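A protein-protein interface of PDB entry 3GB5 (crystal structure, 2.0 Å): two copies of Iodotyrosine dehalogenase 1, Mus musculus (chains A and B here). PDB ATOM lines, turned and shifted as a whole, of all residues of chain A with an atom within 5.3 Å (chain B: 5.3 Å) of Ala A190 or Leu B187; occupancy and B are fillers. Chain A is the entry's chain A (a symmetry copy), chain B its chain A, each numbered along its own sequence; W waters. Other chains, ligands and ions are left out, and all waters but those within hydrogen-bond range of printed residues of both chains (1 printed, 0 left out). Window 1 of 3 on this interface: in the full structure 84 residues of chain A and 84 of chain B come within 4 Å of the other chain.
The side-chain hydroxyl (OG1) of Thr B89 lies within hydrogen-bond range of the backbone carbonyl oxygen (O) of Ala B86 (2.6 Å).
Phe B57 touches Phe A57.
CA of Ala B191 touches CE1 of Phe A57 (3.6 Å).
CD1 of Leu A61 touches CB of Ala B86, 3.9 Å away.
Leu A61 touches Thr B89 (CB to OG1, 3.4 Å).
Gly A186 touches Ile B183 (CA to O, 3.7 Å).
Gly A186 touches Leu B187.
Leu A187 touches Ala B190 (CD2 to CB, 3.8 Å).
Leu A189 touches Ile B183 (CD1 to CG2, 3.7 Å).
Ala A190 touches Phe B57.
Ala A191 touches Phe B57.
Of the printed residues of chain B, Gly A186 touches Ile B183 and Leu B187.
Printed residues of chain B within 4 Å of Leu A189: Pro B91 (3.6 Å) and Ile B183 (3.7 Å).
Ala A190 touches just these residues of chain B: Phe B57 and Leu B187.
Of the printed residues of chain B, Ala A191 touches Phe B57 (3.6 Å).
Of the printed residues of chain A, Ala B86 touches Leu A61 (3.9 Å).
Leu B187 touches just these residues of chain A: Gly A186 (3.3 Å) and Ala A190 (3.8 Å).
Printed residues of chain A within 4 Å of Ala B190: Phe A57 (3.98 Å) and Leu A187 (3.8 Å).
The nearest residue of chain B that does not touch Ala A190 is Ala B190 (5.1 Å).
The nearest printed residue of chain A that does not touch Pro B91 is Gly A186 (6.7 Å).
Of the 14 printed residues of chain A, 8 touch a printed residue of chain B.
Hydrophobic or aromatic side chains of chain A within 4 Å of the printed part of chain B: Phe A57, Leu A61, Leu A187, Leu A189, Ala A190 and Ala A191.
Of the 17 printed residues of chain B, 9 touch a printed residue of chain A.
Among the printed residues, no Asp or Glu carboxylate lies within 4 Å of a Lys or Arg side-chain nitrogen of the other chain.
Phe A57 touches its own counterpart, Phe B57.
Phe A57 touches Ala B190, and with the chains exchanged Ala A190 touches Phe B57.
Gly A186 touches Leu B187, and with the chains exchanged Leu A187 touches Gly B186.
Leu A187 touches Ala B190, and with the chains exchanged Ala A190 touches Leu B187.
Positions printed for both chains: 57, 185, 186, 187, 188, 189, 190, 191 and 192.
Water W1 lies within hydrogen-bond range of the side-chain hydroxyl of Thr B89 (2.8 Å) and the backbone carbonyl oxygen of Leu A61 (2.9 Å).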
ATOM      1  N   PHE A  57      -2.501  -3.515 -26.984  1.00  0.00           N
ATOM      2  CA  PHE A  57      -1.435  -2.965 -26.112  1.00  0.00           C
ATOM      3  C   PHE A  57      -0.310  -4.015 -25.900  1.00  0.00           C
ATOM      4  O   PHE A  57       0.914  -3.703 -25.883  1.00  0.00           O
ATOM      5  CB  PHE A  57      -2.034  -2.540 -24.757  1.00  0.00           C
ATOM      6  CG  PHE A  57      -1.063  -1.791 -23.865  1.00  0.00           C
ATOM      7  CD1 PHE A  57      -0.733  -2.269 -22.607  1.00  0.00           C
ATOM      8  CD2 PHE A  57      -0.465  -0.598 -24.299  1.00  0.00           C
ATOM      9  CE1 PHE A  57       0.174  -1.549 -21.763  1.00  0.00           C
ATOM     10  CE2 PHE A  57       0.423   0.109 -23.462  1.00  0.00           C
ATOM     11  CZ  PHE A  57       0.726  -0.374 -22.193  1.00  0.00           C
ATOM     12  N   LEU A  60       1.724  -4.069 -29.073  1.00  0.00           N
ATOM     13  CA  LEU A  60       2.623  -2.896 -29.083  1.00  0.00           C
ATOM     14  C   LEU A  60       3.868  -3.122 -28.209  1.00  0.00           C
ATOM     15  O   LEU A  60       5.012  -2.869 -28.658  1.00  0.00           O
ATOM     16  CB  LEU A  60       1.886  -1.616 -28.609  1.00  0.00           C
ATOM     17  CG  LEU A  60       2.592  -0.235 -28.527  1.00  0.00           C
ATOM     18  CD1 LEU A  60       1.561   0.863 -28.331  1.00  0.00           C
ATOM     19  CD2 LEU A  60       3.514  -0.128 -27.330  1.00  0.00           C
ATOM     20  N   LEU A  61       3.620  -3.561 -26.962  1.00  0.00           N
ATOM     21  CA  LEU A  61       4.683  -3.786 -26.014  1.00  0.00           C
ATOM     22  C   LEU A  61       5.567  -4.961 -26.430  1.00  0.00           C
ATOM     23  O   LEU A  61       6.757  -4.931 -26.183  1.00  0.00           O
ATOM     24  CB  LEU A  61       4.131  -4.011 -24.595  1.00  0.00           C
ATOM     25  CG  LEU A  61       3.597  -2.771 -23.842  1.00  0.00           C
ATOM     26  CD1 LEU A  61       3.122  -3.247 -22.465  1.00  0.00           C
ATOM     27  CD2 LEU A  61       4.642  -1.624 -23.740  1.00  0.00           C
ATOM     28  N   CYS A 185       9.889   3.113 -13.780  1.00  0.00           N
ATOM     29  CA  CYS A 185      10.737   2.807 -14.928  1.00  0.00           C
ATOM     30  C   CYS A 185      10.032   1.868 -15.914  1.00  0.00           C
ATOM     31  O   CYS A 185      10.261   1.976 -17.092  1.00  0.00           O
ATOM     32  CB  CYS A 185      12.091   2.224 -14.504  1.00  0.00           C
ATOM     33  SG  CYS A 185      13.192   3.370 -13.599  1.00  0.00           S
ATOM     34  N   GLY A 186       9.216   0.925 -15.434  1.00  0.00           N
ATOM     35  CA  GLY A 186       8.361   0.142 -16.355  1.00  0.00           C
ATOM     36  C   GLY A 186       7.403   1.053 -17.134  1.00  0.00           C
ATOM     37  O   GLY A 186       7.246   0.901 -18.329  1.00  0.00           O
ATOM     38  N   LEU A 187       6.744   2.015 -16.461  1.00  0.00           N
ATOM     39  CA  LEU A 187       5.915   2.989 -17.195  1.00  0.00           C
ATOM     40  C   LEU A 187       6.744   3.785 -18.233  1.00  0.00           C
ATOM     41  O   LEU A 187       6.295   4.032 -19.356  1.00  0.00           O
ATOM     42  CB  LEU A 187       5.206   3.949 -16.255  1.00  0.00           C
ATOM     43  CG  LEU A 187       4.221   3.338 -15.236  1.00  0.00           C
ATOM     44  CD1 LEU A 187       3.412   4.447 -14.535  1.00  0.00           C
ATOM     45  CD2 LEU A 187       3.317   2.310 -15.985  1.00  0.00           C
ATOM     46  N   LEU A 188       7.953   4.182 -17.835  1.00  0.00           N
ATOM     47  CA  LEU A 188       8.829   4.948 -18.744  1.00  0.00           C
ATOM     48  C   LEU A 188       9.143   4.108 -19.982  1.00  0.00           C
ATOM     49  O   LEU A 188       9.133   4.612 -21.087  1.00  0.00           O
ATOM     50  CB  LEU A 188      10.169   5.304 -18.038  1.00  0.00           C
ATOM     51  CG  LEU A 188      11.068   6.462 -18.550  1.00  0.00           C
ATOM     52  CD1 LEU A 188      12.346   6.710 -17.685  1.00  0.00           C
ATOM     53  CD2 LEU A 188      11.458   6.312 -19.945  1.00  0.00           C
ATOM     54  N   LEU A 189       9.525   2.839 -19.780  1.00  0.00           N
ATOM     55  CA  LEU A 189       9.817   1.929 -20.915  1.00  0.00           C
ATOM     56  C   LEU A 189       8.632   1.741 -21.880  1.00  0.00           C
ATOM     57  O   LEU A 189       8.808   1.753 -23.120  1.00  0.00           O
ATOM     58  CB  LEU A 189      10.288   0.545 -20.383  1.00  0.00           C
ATOM     59  CG  LEU A 189      11.683   0.564 -19.710  1.00  0.00           C
ATOM     60  CD1 LEU A 189      11.991  -0.724 -18.960  1.00  0.00           C
ATOM     61  CD2 LEU A 189      12.788   0.869 -20.797  1.00  0.00           C
ATOM     62  N   ALA A 190       7.440   1.541 -21.310  1.00  0.00           N
ATOM     63  CA  ALA A 190       6.212   1.469 -22.119  1.00  0.00           C
ATOM     64  C   ALA A 190       5.985   2.755 -22.930  1.00  0.00           C
ATOM     65  O   ALA A 190       5.596   2.704 -24.107  1.00  0.00           O
ATOM     66  CB  ALA A 190       5.006   1.213 -21.232  1.00  0.00           C
ATOM     67  N   ALA A 191       6.187   3.907 -22.282  1.00  0.00           N
ATOM     68  CA  ALA A 191       5.959   5.198 -22.936  1.00  0.00           C
ATOM     69  C   ALA A 191       6.960   5.464 -24.069  1.00  0.00           C
ATOM     70  O   ALA A 191       6.609   6.006 -25.107  1.00  0.00           O
ATOM     71  CB  ALA A 191       5.996   6.358 -21.872  1.00  0.00           C
ATOM     72  N   LEU A 192       8.219   5.061 -23.866  1.00  0.00           N
ATOM     73  CA  LEU A 192       9.213   5.145 -24.949  1.00  0.00           C
ATOM     74  C   LEU A 192       8.805   4.280 -26.158  1.00  0.00           C
ATOM     75  O   LEU A 192       8.846   4.757 -27.299  1.00  0.00           O
ATOM     76  CB  LEU A 192      10.582   4.651 -24.445  1.00  0.00           C
ATOM     77  CG  LEU A 192      11.352   5.578 -23.495  1.00  0.00           C
ATOM     78  CD1 LEU A 192      12.579   4.836 -22.918  1.00  0.00           C
ATOM     79  CD2 LEU A 192      11.861   6.830 -24.269  1.00  0.00           C
ATOM     80  N   GLN A 193       8.401   3.034 -25.894  1.00  0.00           N
ATOM     81  CA  GLN A 193       7.923   2.152 -26.952  1.00  0.00           C
ATOM     82  C   GLN A 193       6.715   2.783 -27.696  1.00  0.00           C
ATOM     83  O   GLN A 193       6.696   2.859 -28.918  1.00  0.00           O
ATOM     84  CB  GLN A 193       7.556   0.784 -26.373  1.00  0.00           C
ATOM     85  CG  GLN A 193       7.121  -0.253 -27.468  1.00  0.00           C
ATOM     86  CD  GLN A 193       8.161  -0.495 -28.590  1.00  0.00           C
ATOM     87  OE1 GLN A 193       9.368  -0.279 -28.416  1.00  0.00           O
ATOM     88  NE2 GLN A 193       7.667  -0.893 -29.774  1.00  0.00           N
ATOM     89  N   ASN A 194       5.723   3.224 -26.938  1.00  0.00           N
ATOM     90  CA  ASN A 194       4.532   3.856 -27.512  1.00  0.00           C
ATOM     91  C   ASN A 194       4.900   5.064 -28.392  1.00  0.00           C
ATOM     92  O   ASN A 194       4.261   5.310 -29.416  1.00  0.00           O
ATOM     93  CB  ASN A 194       3.614   4.313 -26.370  1.00  0.00           C
ATOM     94  CG  ASN A 194       2.333   4.941 -26.879  1.00  0.00           C
ATOM     95  OD1 ASN A 194       1.521   4.264 -27.504  1.00  0.00           O
ATOM     96  ND2 ASN A 194       2.166   6.244 -26.655  1.00  0.00           N
ATOM     97  N   ALA A 195       5.923   5.830 -27.968  1.00  0.00           N
ATOM     98  CA  ALA A 195       6.344   7.034 -28.670  1.00  0.00           C
ATOM     99  C   ALA A 195       7.261   6.785 -29.868  1.00  0.00           C
ATOM    100  O   ALA A 195       7.649   7.734 -30.531  1.00  0.00           O
ATOM    101  CB  ALA A 195       7.036   8.012 -27.681  1.00  0.00           C
ATOM    102  N   PHE B  57      -0.822   9.007 -24.275  1.00  0.00           N
ATOM    103  CA  PHE B  57      -0.481   7.883 -23.368  1.00  0.00           C
ATOM    104  C   PHE B  57      -0.289   8.395 -21.915  1.00  0.00           C
ATOM    105  O   PHE B  57      -0.704   7.755 -20.909  1.00  0.00           O
ATOM    106  CB  PHE B  57       0.798   7.180 -23.863  1.00  0.00           C
ATOM    107  CG  PHE B  57       1.124   5.902 -23.114  1.00  0.00           C
ATOM    108  CD1 PHE B  57       2.325   5.757 -22.438  1.00  0.00           C
ATOM    109  CD2 PHE B  57       0.211   4.839 -23.081  1.00  0.00           C
ATOM    110  CE1 PHE B  57       2.634   4.541 -21.744  1.00  0.00           C
ATOM    111  CE2 PHE B  57       0.522   3.643 -22.401  1.00  0.00           C
ATOM    112  CZ  PHE B  57       1.741   3.505 -21.745  1.00  0.00           C
ATOM    113  N   VAL B  83      -3.199  -8.709 -20.066  1.00  0.00           N
ATOM    114  CA  VAL B  83      -2.419  -7.842 -19.191  1.00  0.00           C
ATOM    115  C   VAL B  83      -1.171  -8.547 -18.669  1.00  0.00           C
ATOM    116  O   VAL B  83      -0.131  -7.899 -18.518  1.00  0.00           O
ATOM    117  CB  VAL B  83      -3.236  -7.162 -18.013  1.00  0.00           C
ATOM    118  CG1 VAL B  83      -4.478  -6.368 -18.583  1.00  0.00           C
ATOM    119  CG2 VAL B  83      -3.695  -8.143 -16.968  1.00  0.00           C
ATOM    120  N   ALA B  86       1.273  -8.759 -21.523  1.00  0.00           N
ATOM    121  CA  ALA B  86       1.909  -7.430 -21.590  1.00  0.00           C
ATOM    122  C   ALA B  86       3.064  -7.338 -20.558  1.00  0.00           C
ATOM    123  O   ALA B  86       4.177  -6.903 -20.910  1.00  0.00           O
ATOM    124  CB  ALA B  86       0.865  -6.270 -21.335  1.00  0.00           C
ATOM    125  N   ALA B  87       2.776  -7.736 -19.307  1.00  0.00           N
ATOM    126  CA  ALA B  87       3.794  -7.721 -18.242  1.00  0.00           C
ATOM    127  C   ALA B  87       5.037  -8.538 -18.606  1.00  0.00           C
ATOM    128  O   ALA B  87       6.180  -8.078 -18.345  1.00  0.00           O
ATOM    129  CB  ALA B  87       3.208  -8.160 -16.872  1.00  0.00           C
ATOM    130  N   THR B  89       6.349  -8.958 -21.384  1.00  0.00           N
ATOM    131  CA  THR B  89       7.192  -8.267 -22.382  1.00  0.00           C
ATOM    132  C   THR B  89       8.422  -7.547 -21.774  1.00  0.00           C
ATOM    133  O   THR B  89       9.181  -6.963 -22.563  1.00  0.00           O
ATOM    134  CB  THR B  89       6.426  -7.377 -23.405  1.00  0.00           C
ATOM    135  OG1 THR B  89       5.898  -6.227 -22.736  1.00  0.00           O
ATOM    136  CG2 THR B  89       5.284  -8.158 -24.104  1.00  0.00           C
ATOM    137  N   ALA B  90       8.588  -7.480 -20.422  1.00  0.00           N
ATOM    138  CA  ALA B  90       9.365  -6.455 -19.699  1.00  0.00           C
ATOM    139  C   ALA B  90      10.777  -6.906 -20.222  1.00  0.00           C
ATOM    140  O   ALA B  90      11.003  -8.146 -20.404  1.00  0.00           O
ATOM    141  CB  ALA B  90       9.292  -6.637 -18.180  1.00  0.00           C
ATOM    142  N   PRO B  91      11.818  -6.036 -20.167  1.00  0.00           N
ATOM    143  CA  PRO B  91      13.212  -6.447 -19.998  1.00  0.00           C
ATOM    144  C   PRO B  91      13.545  -7.212 -18.718  1.00  0.00           C
ATOM    145  O   PRO B  91      12.817  -7.122 -17.744  1.00  0.00           O
ATOM    146  CB  PRO B  91      13.977  -5.123 -20.139  1.00  0.00           C
ATOM    147  CG  PRO B  91      13.056  -4.150 -19.347  1.00  0.00           C
ATOM    148  CD  PRO B  91      11.647  -4.582 -19.872  1.00  0.00           C
ATOM    149  N   ILE B 183       9.701  -3.840 -12.795  1.00  0.00           N
ATOM    150  CA  ILE B 183       9.477  -3.213 -14.110  1.00  0.00           C
ATOM    151  C   ILE B 183       8.281  -3.910 -14.809  1.00  0.00           C
ATOM    152  O   ILE B 183       7.374  -3.242 -15.357  1.00  0.00           O
ATOM    153  CB  ILE B 183      10.760  -3.291 -14.992  1.00  0.00           C
ATOM    154  CG1 ILE B 183      11.808  -2.226 -14.532  1.00  0.00           C
ATOM    155  CG2 ILE B 183      10.422  -3.021 -16.474  1.00  0.00           C
ATOM    156  CD1 ILE B 183      13.273  -2.440 -15.113  1.00  0.00           C
ATOM    157  N   ALA B 184       8.293  -5.249 -14.807  1.00  0.00           N
ATOM    158  CA  ALA B 184       7.151  -6.041 -15.340  1.00  0.00           C
ATOM    159  C   ALA B 184       5.828  -5.641 -14.661  1.00  0.00           C
ATOM    160  O   ALA B 184       4.794  -5.572 -15.311  1.00  0.00           O
ATOM    161  CB  ALA B 184       7.406  -7.551 -15.181  1.00  0.00           C
ATOM    162  N   CYS B 185       5.872  -5.402 -13.348  1.00  0.00           N
ATOM    163  CA  CYS B 185       4.677  -4.955 -12.639  1.00  0.00           C
ATOM    164  C   CYS B 185       4.248  -3.553 -13.087  1.00  0.00           C
ATOM    165  O   CYS B 185       3.075  -3.277 -13.102  1.00  0.00           O
ATOM    166  CB  CYS B 185       4.862  -4.999 -11.116  1.00  0.00           C
ATOM    167  SG  CYS B 185       5.047  -6.670 -10.396  1.00  0.00           S
ATOM    168  N   GLY B 186       5.190  -2.663 -13.408  1.00  0.00           N
ATOM    169  CA  GLY B 186       4.815  -1.378 -14.042  1.00  0.00           C
ATOM    170  C   GLY B 186       4.100  -1.606 -15.379  1.00  0.00           C
ATOM    171  O   GLY B 186       3.095  -0.981 -15.653  1.00  0.00           O
ATOM    172  N   LEU B 187       4.614  -2.510 -16.235  1.00  0.00           N
ATOM    173  CA  LEU B 187       3.885  -2.848 -17.472  1.00  0.00           C
ATOM    174  C   LEU B 187       2.471  -3.406 -17.173  1.00  0.00           C
ATOM    175  O   LEU B 187       1.496  -3.072 -17.851  1.00  0.00           O
ATOM    176  CB  LEU B 187       4.657  -3.834 -18.331  1.00  0.00           C
ATOM    177  CG  LEU B 187       6.042  -3.386 -18.844  1.00  0.00           C
ATOM    178  CD1 LEU B 187       6.580  -4.384 -19.888  1.00  0.00           C
ATOM    179  CD2 LEU B 187       5.911  -1.935 -19.405  1.00  0.00           C
ATOM    180  N   LEU B 188       2.383  -4.259 -16.153  1.00  0.00           N
ATOM    181  CA  LEU B 188       1.084  -4.852 -15.780  1.00  0.00           C
ATOM    182  C   LEU B 188       0.113  -3.745 -15.373  1.00  0.00           C
ATOM    183  O   LEU B 188      -1.044  -3.774 -15.743  1.00  0.00           O
ATOM    184  CB  LEU B 188       1.254  -5.825 -14.576  1.00  0.00           C
ATOM    185  CG  LEU B 188       0.195  -6.918 -14.266  1.00  0.00           C
ATOM    186  CD1 LEU B 188       0.561  -7.835 -13.054  1.00  0.00           C
ATOM    187  CD2 LEU B 188      -1.145  -6.381 -14.071  1.00  0.00           C
ATOM    188  N   LEU B 189       0.566  -2.817 -14.518  1.00  0.00           N
ATOM    189  CA  LEU B 189      -0.284  -1.678 -14.090  1.00  0.00           C
ATOM    190  C   LEU B 189      -0.783  -0.804 -15.254  1.00  0.00           C
ATOM    191  O   LEU B 189      -1.970  -0.404 -15.292  1.00  0.00           O
ATOM    192  CB  LEU B 189       0.479  -0.798 -13.060  1.00  0.00           C
ATOM    193  CG  LEU B 189       0.704  -1.477 -11.685  1.00  0.00           C
ATOM    194  CD1 LEU B 189       1.685  -0.715 -10.805  1.00  0.00           C
ATOM    195  CD2 LEU B 189      -0.687  -1.667 -10.959  1.00  0.00           C
ATOM    196  N   ALA B 190       0.125  -0.489 -16.181  1.00  0.00           N
ATOM    197  CA  ALA B 190      -0.253   0.238 -17.403  1.00  0.00           C
ATOM    198  C   ALA B 190      -1.311  -0.524 -18.217  1.00  0.00           C
ATOM    199  O   ALA B 190      -2.265   0.075 -18.739  1.00  0.00           O
ATOM    200  CB  ALA B 190       0.967   0.488 -18.273  1.00  0.00           C
ATOM    201  N   ALA B 191      -1.114  -1.838 -18.361  1.00  0.00           N
ATOM    202  CA  ALA B 191      -2.030  -2.664 -19.153  1.00  0.00           C
ATOM    203  C   ALA B 191      -3.422  -2.770 -18.514  1.00  0.00           C
ATOM    204  O   ALA B 191      -4.433  -2.756 -19.200  1.00  0.00           O
ATOM    205  CB  ALA B 191      -1.409  -4.092 -19.386  1.00  0.00           C
ATOM    206  N   LEU B 192      -3.465  -2.863 -17.181  1.00  0.00           N
ATOM    207  CA  LEU B 192      -4.755  -2.826 -16.472  1.00  0.00           C
ATOM    208  C   LEU B 192      -5.493  -1.494 -16.712  1.00  0.00           C
ATOM    209  O   LEU B 192      -6.689  -1.500 -17.032  1.00  0.00           O
ATOM    210  CB  LEU B 192      -4.528  -2.983 -14.957  1.00  0.00           C
ATOM    211  CG  LEU B 192      -4.145  -4.380 -14.450  1.00  0.00           C
ATOM    212  CD1 LEU B 192      -3.739  -4.305 -12.961  1.00  0.00           C
ATOM    213  CD2 LEU B 192      -5.364  -5.343 -14.573  1.00  0.00           C
HETATM  214  O   HOH W   1       7.650  -4.192 -23.514  1.00  0.00           O
